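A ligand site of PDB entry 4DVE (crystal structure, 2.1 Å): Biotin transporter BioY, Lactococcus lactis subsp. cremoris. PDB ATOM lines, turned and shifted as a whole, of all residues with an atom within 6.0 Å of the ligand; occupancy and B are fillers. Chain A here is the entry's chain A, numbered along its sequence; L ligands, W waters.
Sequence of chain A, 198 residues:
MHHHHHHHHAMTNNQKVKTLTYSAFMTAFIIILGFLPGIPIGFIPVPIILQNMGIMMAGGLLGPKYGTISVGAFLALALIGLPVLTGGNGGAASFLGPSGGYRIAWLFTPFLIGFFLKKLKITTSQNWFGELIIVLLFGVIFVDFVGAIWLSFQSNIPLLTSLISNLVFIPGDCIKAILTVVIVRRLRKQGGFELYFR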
ATOM      1  N   VAL A  46      -7.118   3.567 -15.723  1.00  0.00           N
ATOM      2  CA  VAL A  46      -5.911   3.561 -14.881  1.00  0.00           C
ATOM      3  C   VAL A  46      -6.197   2.588 -13.744  1.00  0.00           C
ATOM      4  O   VAL A  46      -7.184   2.742 -13.026  1.00  0.00           O
ATOM      5  CB  VAL A  46      -5.593   4.974 -14.317  1.00  0.00           C
ATOM      6  CG1 VAL A  46      -4.398   4.976 -13.360  1.00  0.00           C
ATOM      7  CG2 VAL A  46      -5.389   5.962 -15.449  1.00  0.00           C
ATOM      8  N   PRO A  47      -5.334   1.576 -13.566  1.00  0.00           N
ATOM      9  CA  PRO A  47      -5.521   0.590 -12.513  1.00  0.00           C
ATOM     10  C   PRO A  47      -4.983   1.002 -11.129  1.00  0.00           C
ATOM     11  O   PRO A  47      -4.098   1.865 -10.997  1.00  0.00           O
ATOM     12  CB  PRO A  47      -4.733  -0.615 -13.040  1.00  0.00           C
ATOM     13  CG  PRO A  47      -3.588  -0.014 -13.763  1.00  0.00           C
ATOM     14  CD  PRO A  47      -4.177   1.231 -14.432  1.00  0.00           C
ATOM     15  N   ILE A  48      -5.487   0.334 -10.102  1.00  0.00           N
ATOM     16  CA  ILE A  48      -4.837   0.379  -8.809  1.00  0.00           C
ATOM     17  C   ILE A  48      -3.614  -0.549  -8.914  1.00  0.00           C
ATOM     18  O   ILE A  48      -3.688  -1.665  -9.473  1.00  0.00           O
ATOM     19  CB  ILE A  48      -5.777  -0.112  -7.705  1.00  0.00           C
ATOM     20  CG1 ILE A  48      -7.002   0.839  -7.562  1.00  0.00           C
ATOM     21  CG2 ILE A  48      -5.033  -0.320  -6.390  1.00  0.00           C
ATOM     22  CD1 ILE A  48      -8.149   0.269  -6.714  1.00  0.00           C
ATOM     23  N   ILE A  49      -2.492  -0.070  -8.384  1.00  0.00           N
ATOM     24  CA  ILE A  49      -1.221  -0.779  -8.457  1.00  0.00           C
ATOM     25  C   ILE A  49      -0.526  -0.745  -7.105  1.00  0.00           C
ATOM     26  O   ILE A  49      -0.976  -0.062  -6.156  1.00  0.00           O
ATOM     27  CB  ILE A  49      -0.270  -0.153  -9.527  1.00  0.00           C
ATOM     28  CG1 ILE A  49       0.132   1.290  -9.165  1.00  0.00           C
ATOM     29  CG2 ILE A  49      -0.919  -0.145 -10.932  1.00  0.00           C
ATOM     30  CD1 ILE A  49       1.295   1.828  -9.975  1.00  0.00           C
ATOM     31  N   LEU A  50       0.585  -1.447  -7.016  1.00  0.00           N
ATOM     32  CA  LEU A  50       1.451  -1.358  -5.849  1.00  0.00           C
ATOM     33  C   LEU A  50       2.757  -0.604  -6.139  1.00  0.00           C
ATOM     34  O   LEU A  50       3.386  -0.106  -5.217  1.00  0.00           O
ATOM     35  CB  LEU A  50       1.759  -2.764  -5.319  1.00  0.00           C
ATOM     36  CG  LEU A  50       2.513  -2.866  -3.995  1.00  0.00           C
ATOM     37  CD1 LEU A  50       1.825  -2.095  -2.856  1.00  0.00           C
ATOM     38  CD2 LEU A  50       2.727  -4.347  -3.616  1.00  0.00           C
ATOM     39  N   GLN A  51       3.140  -0.489  -7.418  1.00  0.00           N
ATOM     40  CA  GLN A  51       4.502  -0.057  -7.778  1.00  0.00           C
ATOM     41  C   GLN A  51       4.855   1.382  -7.343  1.00  0.00           C
ATOM     42  O   GLN A  51       6.035   1.682  -7.061  1.00  0.00           O
ATOM     43  CB  GLN A  51       4.710  -0.307  -9.277  1.00  0.00           C
ATOM     44  CG  GLN A  51       6.051   0.039  -9.839  1.00  0.00           C
ATOM     45  CD  GLN A  51       6.275  -0.528 -11.246  1.00  0.00           C
ATOM     46  OE1 GLN A  51       7.144  -1.401 -11.445  1.00  0.00           O
ATOM     47  NE2 GLN A  51       5.532  -0.009 -12.211  1.00  0.00           N
ATOM     48  N   ASN A  52       3.860   2.275  -7.283  1.00  0.00           N
ATOM     49  CA  ASN A  52       4.112   3.620  -6.831  1.00  0.00           C
ATOM     50  C   ASN A  52       4.628   3.698  -5.384  1.00  0.00           C
ATOM     51  O   ASN A  52       5.266   4.676  -5.016  1.00  0.00           O
ATOM     52  CB  ASN A  52       2.913   4.562  -7.059  1.00  0.00           C
ATOM     53  CG  ASN A  52       1.681   4.148  -6.310  1.00  0.00           C
ATOM     54  OD1 ASN A  52       1.362   2.966  -6.247  1.00  0.00           O
ATOM     55  ND2 ASN A  52       0.950   5.135  -5.750  1.00  0.00           N
ATOM     56  N   LEU A  85       6.990  -2.093 -16.061  1.00  0.00           N
ATOM     57  CA  LEU A  85       5.807  -1.449 -15.462  1.00  0.00           C
ATOM     58  C   LEU A  85       4.816  -2.538 -15.114  1.00  0.00           C
ATOM     59  O   LEU A  85       4.856  -3.631 -15.689  1.00  0.00           O
ATOM     60  CB  LEU A  85       5.157  -0.454 -16.434  1.00  0.00           C
ATOM     61  CG  LEU A  85       6.075   0.691 -16.890  1.00  0.00           C
ATOM     62  CD1 LEU A  85       5.421   1.506 -18.009  1.00  0.00           C
ATOM     63  CD2 LEU A  85       6.479   1.558 -15.708  1.00  0.00           C
ATOM     64  N   THR A  86       3.916  -2.225 -14.188  1.00  0.00           N
ATOM     65  CA  THR A  86       2.864  -3.149 -13.726  1.00  0.00           C
ATOM     66  C   THR A  86       2.206  -3.996 -14.835  1.00  0.00           C
ATOM     67  O   THR A  86       1.763  -3.478 -15.864  1.00  0.00           O
ATOM     68  CB  THR A  86       1.788  -2.360 -12.949  1.00  0.00           C
ATOM     69  OG1 THR A  86       2.381  -1.772 -11.775  1.00  0.00           O
ATOM     70  CG2 THR A  86       0.612  -3.297 -12.584  1.00  0.00           C
ATOM     71  N   ASN A  89       4.377  -4.291 -18.691  1.00  0.00           N
ATOM     72  CA  ASN A  89       4.243  -3.240 -19.684  1.00  0.00           C
ATOM     73  C   ASN A  89       5.490  -2.379 -19.781  1.00  0.00           C
ATOM     74  O   ASN A  89       6.310  -2.324 -18.854  1.00  0.00           O
ATOM     75  CB  ASN A  89       3.014  -2.371 -19.380  1.00  0.00           C
ATOM     76  CG  ASN A  89       1.702  -3.096 -19.689  1.00  0.00           C
ATOM     77  OD1 ASN A  89       1.465  -3.471 -20.813  1.00  0.00           O
ATOM     78  ND2 ASN A  89       0.867  -3.296 -18.677  1.00  0.00           N
ATOM     79  N   SER A  94       3.937   3.812 -24.568  1.00  0.00           N
ATOM     80  CA  SER A  94       3.029   3.711 -23.407  1.00  0.00           C
ATOM     81  C   SER A  94       3.066   4.938 -22.466  1.00  0.00           C
ATOM     82  O   SER A  94       2.148   5.148 -21.693  1.00  0.00           O
ATOM     83  CB  SER A  94       3.339   2.465 -22.571  1.00  0.00           C
ATOM     84  OG  SER A  94       4.544   2.641 -21.826  1.00  0.00           O
ATOM     85  N   SER A  99      -1.905   6.694 -18.352  1.00  0.00           N
ATOM     86  CA  SER A  99      -1.200   6.731 -17.097  1.00  0.00           C
ATOM     87  C   SER A  99       0.149   7.467 -17.187  1.00  0.00           C
ATOM     88  O   SER A  99       0.923   7.469 -16.227  1.00  0.00           O
ATOM     89  CB  SER A  99      -1.021   5.305 -16.575  1.00  0.00           C
ATOM     90  OG  SER A  99      -0.008   4.601 -17.304  1.00  0.00           O
ATOM     91  N   GLY A 100       0.414   8.135 -18.312  1.00  0.00           N
ATOM     92  CA  GLY A 100       1.689   8.829 -18.530  1.00  0.00           C
ATOM     93  C   GLY A 100       2.034   9.888 -17.498  1.00  0.00           C
ATOM     94  O   GLY A 100       3.192  10.012 -17.061  1.00  0.00           O
ATOM     95  N   TYR A 102       1.160  10.128 -14.274  1.00  0.00           N
ATOM     96  CA  TYR A 102       1.591   9.584 -13.013  1.00  0.00           C
ATOM     97  C   TYR A 102       3.080   9.223 -13.084  1.00  0.00           C
ATOM     98  O   TYR A 102       3.868   9.526 -12.176  1.00  0.00           O
ATOM     99  CB  TYR A 102       0.791   8.333 -12.624  1.00  0.00           C
ATOM    100  CG  TYR A 102      -0.704   8.529 -12.558  1.00  0.00           C
ATOM    101  CD1 TYR A 102      -1.338   8.996 -11.383  1.00  0.00           C
ATOM    102  CD2 TYR A 102      -1.504   8.243 -13.682  1.00  0.00           C
ATOM    103  CE1 TYR A 102      -2.722   9.130 -11.333  1.00  0.00           C
ATOM    104  CE2 TYR A 102      -2.884   8.398 -13.639  1.00  0.00           C
ATOM    105  CZ  TYR A 102      -3.497   8.853 -12.472  1.00  0.00           C
ATOM    106  OH  TYR A 102      -4.881   9.009 -12.482  1.00  0.00           O
ATOM    107  N   ARG A 103       3.459   8.609 -14.197  1.00  0.00           N
ATOM    108  CA  ARG A 103       4.839   8.152 -14.444  1.00  0.00           C
ATOM    109  C   ARG A 103       5.872   9.267 -14.524  1.00  0.00           C
ATOM    110  O   ARG A 103       6.978   9.147 -13.984  1.00  0.00           O
ATOM    111  CB  ARG A 103       4.872   7.289 -15.709  1.00  0.00           C
ATOM    112  CG  ARG A 103       4.346   5.912 -15.358  1.00  0.00           C
ATOM    113  CD  ARG A 103       3.435   5.309 -16.370  1.00  0.00           C
ATOM    114  NE  ARG A 103       4.095   5.034 -17.602  1.00  0.00           N
ATOM    115  CZ  ARG A 103       3.547   4.338 -18.585  1.00  0.00           C
ATOM    116  NH1 ARG A 103       4.270   4.112 -19.674  1.00  0.00           N
ATOM    117  NH2 ARG A 103       2.324   3.859 -18.495  1.00  0.00           N
ATOM    118  N   TRP A 106       6.406  10.580 -11.142  1.00  0.00           N
ATOM    119  CA  TRP A 106       7.287   9.672 -10.369  1.00  0.00           C
ATOM    120  C   TRP A 106       8.753  10.059 -10.429  1.00  0.00           C
ATOM    121  O   TRP A 106       9.439   9.924  -9.449  1.00  0.00           O
ATOM    122  CB  TRP A 106       7.173   8.240 -10.810  1.00  0.00           C
ATOM    123  CG  TRP A 106       5.882   7.532 -10.532  1.00  0.00           C
ATOM    124  CD1 TRP A 106       4.788   7.964  -9.768  1.00  0.00           C
ATOM    125  CD2 TRP A 106       5.501   6.220 -11.042  1.00  0.00           C
ATOM    126  NE1 TRP A 106       3.812   7.023  -9.769  1.00  0.00           N
ATOM    127  CE2 TRP A 106       4.173   5.941 -10.516  1.00  0.00           C
ATOM    128  CE3 TRP A 106       6.133   5.266 -11.831  1.00  0.00           C
ATOM    129  CZ2 TRP A 106       3.516   4.751 -10.786  1.00  0.00           C
ATOM    130  CZ3 TRP A 106       5.471   4.067 -12.074  1.00  0.00           C
ATOM    131  CH2 TRP A 106       4.187   3.824 -11.588  1.00  0.00           C
ATOM    132  N   VAL A 143       1.605  13.359  -7.326  1.00  0.00           N
ATOM    133  CA  VAL A 143       1.493  12.297  -8.338  1.00  0.00           C
ATOM    134  C   VAL A 143       0.077  12.142  -8.933  1.00  0.00           C
ATOM    135  O   VAL A 143      -0.087  12.162 -10.181  1.00  0.00           O
ATOM    136  CB  VAL A 143       2.033  10.966  -7.799  1.00  0.00           C
ATOM    137  CG1 VAL A 143       1.695   9.778  -8.730  1.00  0.00           C
ATOM    138  CG2 VAL A 143       3.552  11.090  -7.530  1.00  0.00           C
ATOM    139  N   ASP A 144      -0.934  12.033  -8.060  1.00  0.00           N
ATOM    140  CA  ASP A 144      -2.299  11.778  -8.490  1.00  0.00           C
ATOM    141  C   ASP A 144      -2.917  12.999  -9.203  1.00  0.00           C
ATOM    142  O   ASP A 144      -3.648  12.856 -10.173  1.00  0.00           O
ATOM    143  CB  ASP A 144      -3.182  11.265  -7.314  1.00  0.00           C
ATOM    144  CG  ASP A 144      -2.696   9.901  -6.744  1.00  0.00           C
ATOM    145  OD1 ASP A 144      -1.681   9.355  -7.227  1.00  0.00           O
ATOM    146  OD2 ASP A 144      -3.294   9.400  -5.738  1.00  0.00           O
ATOM    147  N   ASN A 166     -10.079   9.957  -9.504  1.00  0.00           N
ATOM    148  CA  ASN A 166      -8.813   9.681  -8.844  1.00  0.00           C
ATOM    149  C   ASN A 166      -8.895   9.505  -7.324  1.00  0.00           C
ATOM    150  O   ASN A 166      -7.969   9.013  -6.726  1.00  0.00           O
ATOM    151  CB  ASN A 166      -7.770  10.717  -9.223  1.00  0.00           C
ATOM    152  CG  ASN A 166      -7.032  10.320 -10.490  1.00  0.00           C
ATOM    153  OD1 ASN A 166      -7.580  10.396 -11.624  1.00  0.00           O
ATOM    154  ND2 ASN A 166      -5.858   9.800 -10.318  1.00  0.00           N
ATOM    155  N   PHE A 169      -8.028   6.133  -5.841  1.00  0.00           N
ATOM    156  CA  PHE A 169      -6.638   5.774  -5.520  1.00  0.00           C
ATOM    157  C   PHE A 169      -6.190   6.143  -4.121  1.00  0.00           C
ATOM    158  O   PHE A 169      -5.173   5.619  -3.654  1.00  0.00           O
ATOM    159  CB  PHE A 169      -5.650   6.360  -6.536  1.00  0.00           C
ATOM    160  CG  PHE A 169      -5.915   5.919  -7.940  1.00  0.00           C
ATOM    161  CD1 PHE A 169      -6.051   4.560  -8.238  1.00  0.00           C
ATOM    162  CD2 PHE A 169      -6.093   6.845  -8.953  1.00  0.00           C
ATOM    163  CE1 PHE A 169      -6.367   4.139  -9.530  1.00  0.00           C
ATOM    164  CE2 PHE A 169      -6.393   6.433 -10.239  1.00  0.00           C
ATOM    165  CZ  PHE A 169      -6.536   5.085 -10.535  1.00  0.00           C
ATOM    166  N   ASP A 173      -3.312   4.535  -1.762  1.00  0.00           N
ATOM    167  CA  ASP A 173      -2.120   5.394  -1.741  1.00  0.00           C
ATOM    168  C   ASP A 173      -1.719   5.829  -0.314  1.00  0.00           C
ATOM    169  O   ASP A 173      -0.503   5.918  -0.015  1.00  0.00           O
ATOM    170  CB  ASP A 173      -2.233   6.576  -2.691  1.00  0.00           C
ATOM    171  CG  ASP A 173      -2.172   6.160  -4.169  1.00  0.00           C
ATOM    172  OD1 ASP A 173      -1.874   4.970  -4.463  1.00  0.00           O
ATOM    173  OD2 ASP A 173      -2.458   7.012  -5.076  1.00  0.00           O
ATOM    174  N   LYS A 176      -0.036   2.896   1.301  1.00  0.00           N
ATOM    175  CA  LYS A 176       1.330   2.830   0.753  1.00  0.00           C
ATOM    176  C   LYS A 176       2.234   3.849   1.406  1.00  0.00           C
ATOM    177  O   LYS A 176       3.379   3.550   1.687  1.00  0.00           O
ATOM    178  CB  LYS A 176       1.388   3.025  -0.764  1.00  0.00           C
ATOM    179  CG  LYS A 176       0.715   1.904  -1.568  1.00  0.00           C
ATOM    180  CD  LYS A 176       0.459   2.345  -3.015  1.00  0.00           C
ATOM    181  CE  LYS A 176      -0.835   1.795  -3.594  1.00  0.00           C
ATOM    182  NZ  LYS A 176      -1.135   2.370  -4.927  1.00  0.00           N
HETATM  183  C1  LIG L   1       1.599   2.335 -15.397  1.00  0.00           C
HETATM  184  O1  LIG L   1       2.168   1.276 -15.040  1.00  0.00           O
HETATM  185  O2  LIG L   1       1.267   2.491 -16.584  1.00  0.00           O
HETATM  186  C2  LIG L   1       1.332   3.486 -14.396  1.00  0.00           C
HETATM  187  C3  LIG L   1       0.062   3.268 -13.571  1.00  0.00           C
HETATM  188  C4  LIG L   1      -0.191   4.487 -12.643  1.00  0.00           C
HETATM  189  C5  LIG L   1      -1.266   4.170 -11.588  1.00  0.00           C
HETATM  190  C6  LIG L   1      -1.505   5.323 -10.633  1.00  0.00           C
HETATM  191  S1  LIG L   1      -0.076   5.603  -9.582  1.00  0.00           S
HETATM  192  C7  LIG L   1      -1.062   6.545  -8.440  1.00  0.00           C
HETATM  193  C8  LIG L   1      -2.481   5.912  -8.403  1.00  0.00           C
HETATM  194  N1  LIG L   1      -2.567   4.897  -7.386  1.00  0.00           N
HETATM  195  C9  LIG L   1      -2.753   3.678  -7.881  1.00  0.00           C
HETATM  196  O3  LIG L   1      -2.875   2.645  -7.220  1.00  0.00           O
HETATM  197  N2  LIG L   1      -2.812   3.768  -9.222  1.00  0.00           N
HETATM  198  C10 LIG L   1      -2.693   5.124  -9.703  1.00  0.00           C
HETATM  199  O   HOH W   1       1.361  -0.864 -16.511  1.00  0.00           O
HETATM  200  O   HOH W   2      -4.425   3.011  -4.765  1.00  0.00           O
HETATM  201  O   HOH W   3       3.159   0.561 -12.797  1.00  0.00           O
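Water W3 lies within hydrogen-bond range of NE2 of Gln 51 (2.5 Å), O1 of the ligand (2.6 Å) and OG1 of Thr 86 (2.7 Å).
Water W1 lies within hydrogen-bond range of O1 of the ligand (2.7 Å), O of Thr 86 (2.7 Å) and ND2 of Asn 89 (3.3 Å).
The backbone carbonyl oxygen (O) of Pro 47 sits at hydrogen-bond distance from a nitrogen (N2) of the ligand (2.9 Å).
An oxygen (O3) of the ligand is in hydrogen-bond range of the backbone NH (N) of Ile 49.
A nitrogen (N1) of the ligand is in hydrogen-bond range of the side-chain carboxylate (OD1) of Asp 173 (3.0 Å).
The side-chain amino group of Lys 176 is in hydrogen-bond range of an oxygen (O3) of the ligand, at 2.9 Å.
The guanidinium group (NH2) of Arg 103 lies within salt-bridge range of an oxygen (O2) of the ligand, at 2.6 Å.
OG of Ser 99 lies within hydrogen-bond range of O2 of the ligand (2.6 Å).
OD2 of Asp 144 sits close to OD2 of Asp 173 (2.6 Å).
The backbone carbonyl oxygen (O) of Tyr 102 lies close to the indole nitrogen (NE1) of Trp 106 (3.5 Å).
The side-chain hydroxyl (OG) of Ser 99 sits at hydrogen-bond distance from the guanidinium group (NH2) of Arg 103, at 2.7 Å.
O of Ile 49 is in hydrogen-bond range of NZ of Lys 176 (2.7 Å).
NZ of Lys 176 lies within salt-bridge range of OD1 of Asp 173, at 2.7 Å.
The side-chain hydroxyl (OH) of Tyr 102 is in hydrogen-bond range of the side-chain amide nitrogen (ND2) of Asn 166.
The side-chain amide oxygen (OD1) of Asn 52 is in hydrogen-bond range of the side-chain amino group (NZ) of Lys 176, at 2.9 Å.
The side-chain amide nitrogen (ND2) of Asn 52 is in hydrogen-bond range of the side-chain carboxylate (OD1) of Asp 173.
Val 46 touches the ligand (CG1 to C5, 3.7 Å).
CA of Ile 48 touches O3 of the ligand, 3.4 Å away.
Asn 52 touches the ligand (ND2 to C7, 3.6 Å).
Leu 85 touches the ligand.
CD1 of Tyr 102 touches C6 of the ligand (3.8 Å).
Trp 106 touches the ligand (CZ2 to S1, 3.9 Å).
Asp 144 touches the ligand.
Phe 169 touches the ligand (CD1 to C9, 3.4 Å).
Of the 22 residues printed, 14 come within 4 Å of the ligand.
The nearest printed residue that does not touch the ligand is Thr 86 (4.005 Å).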
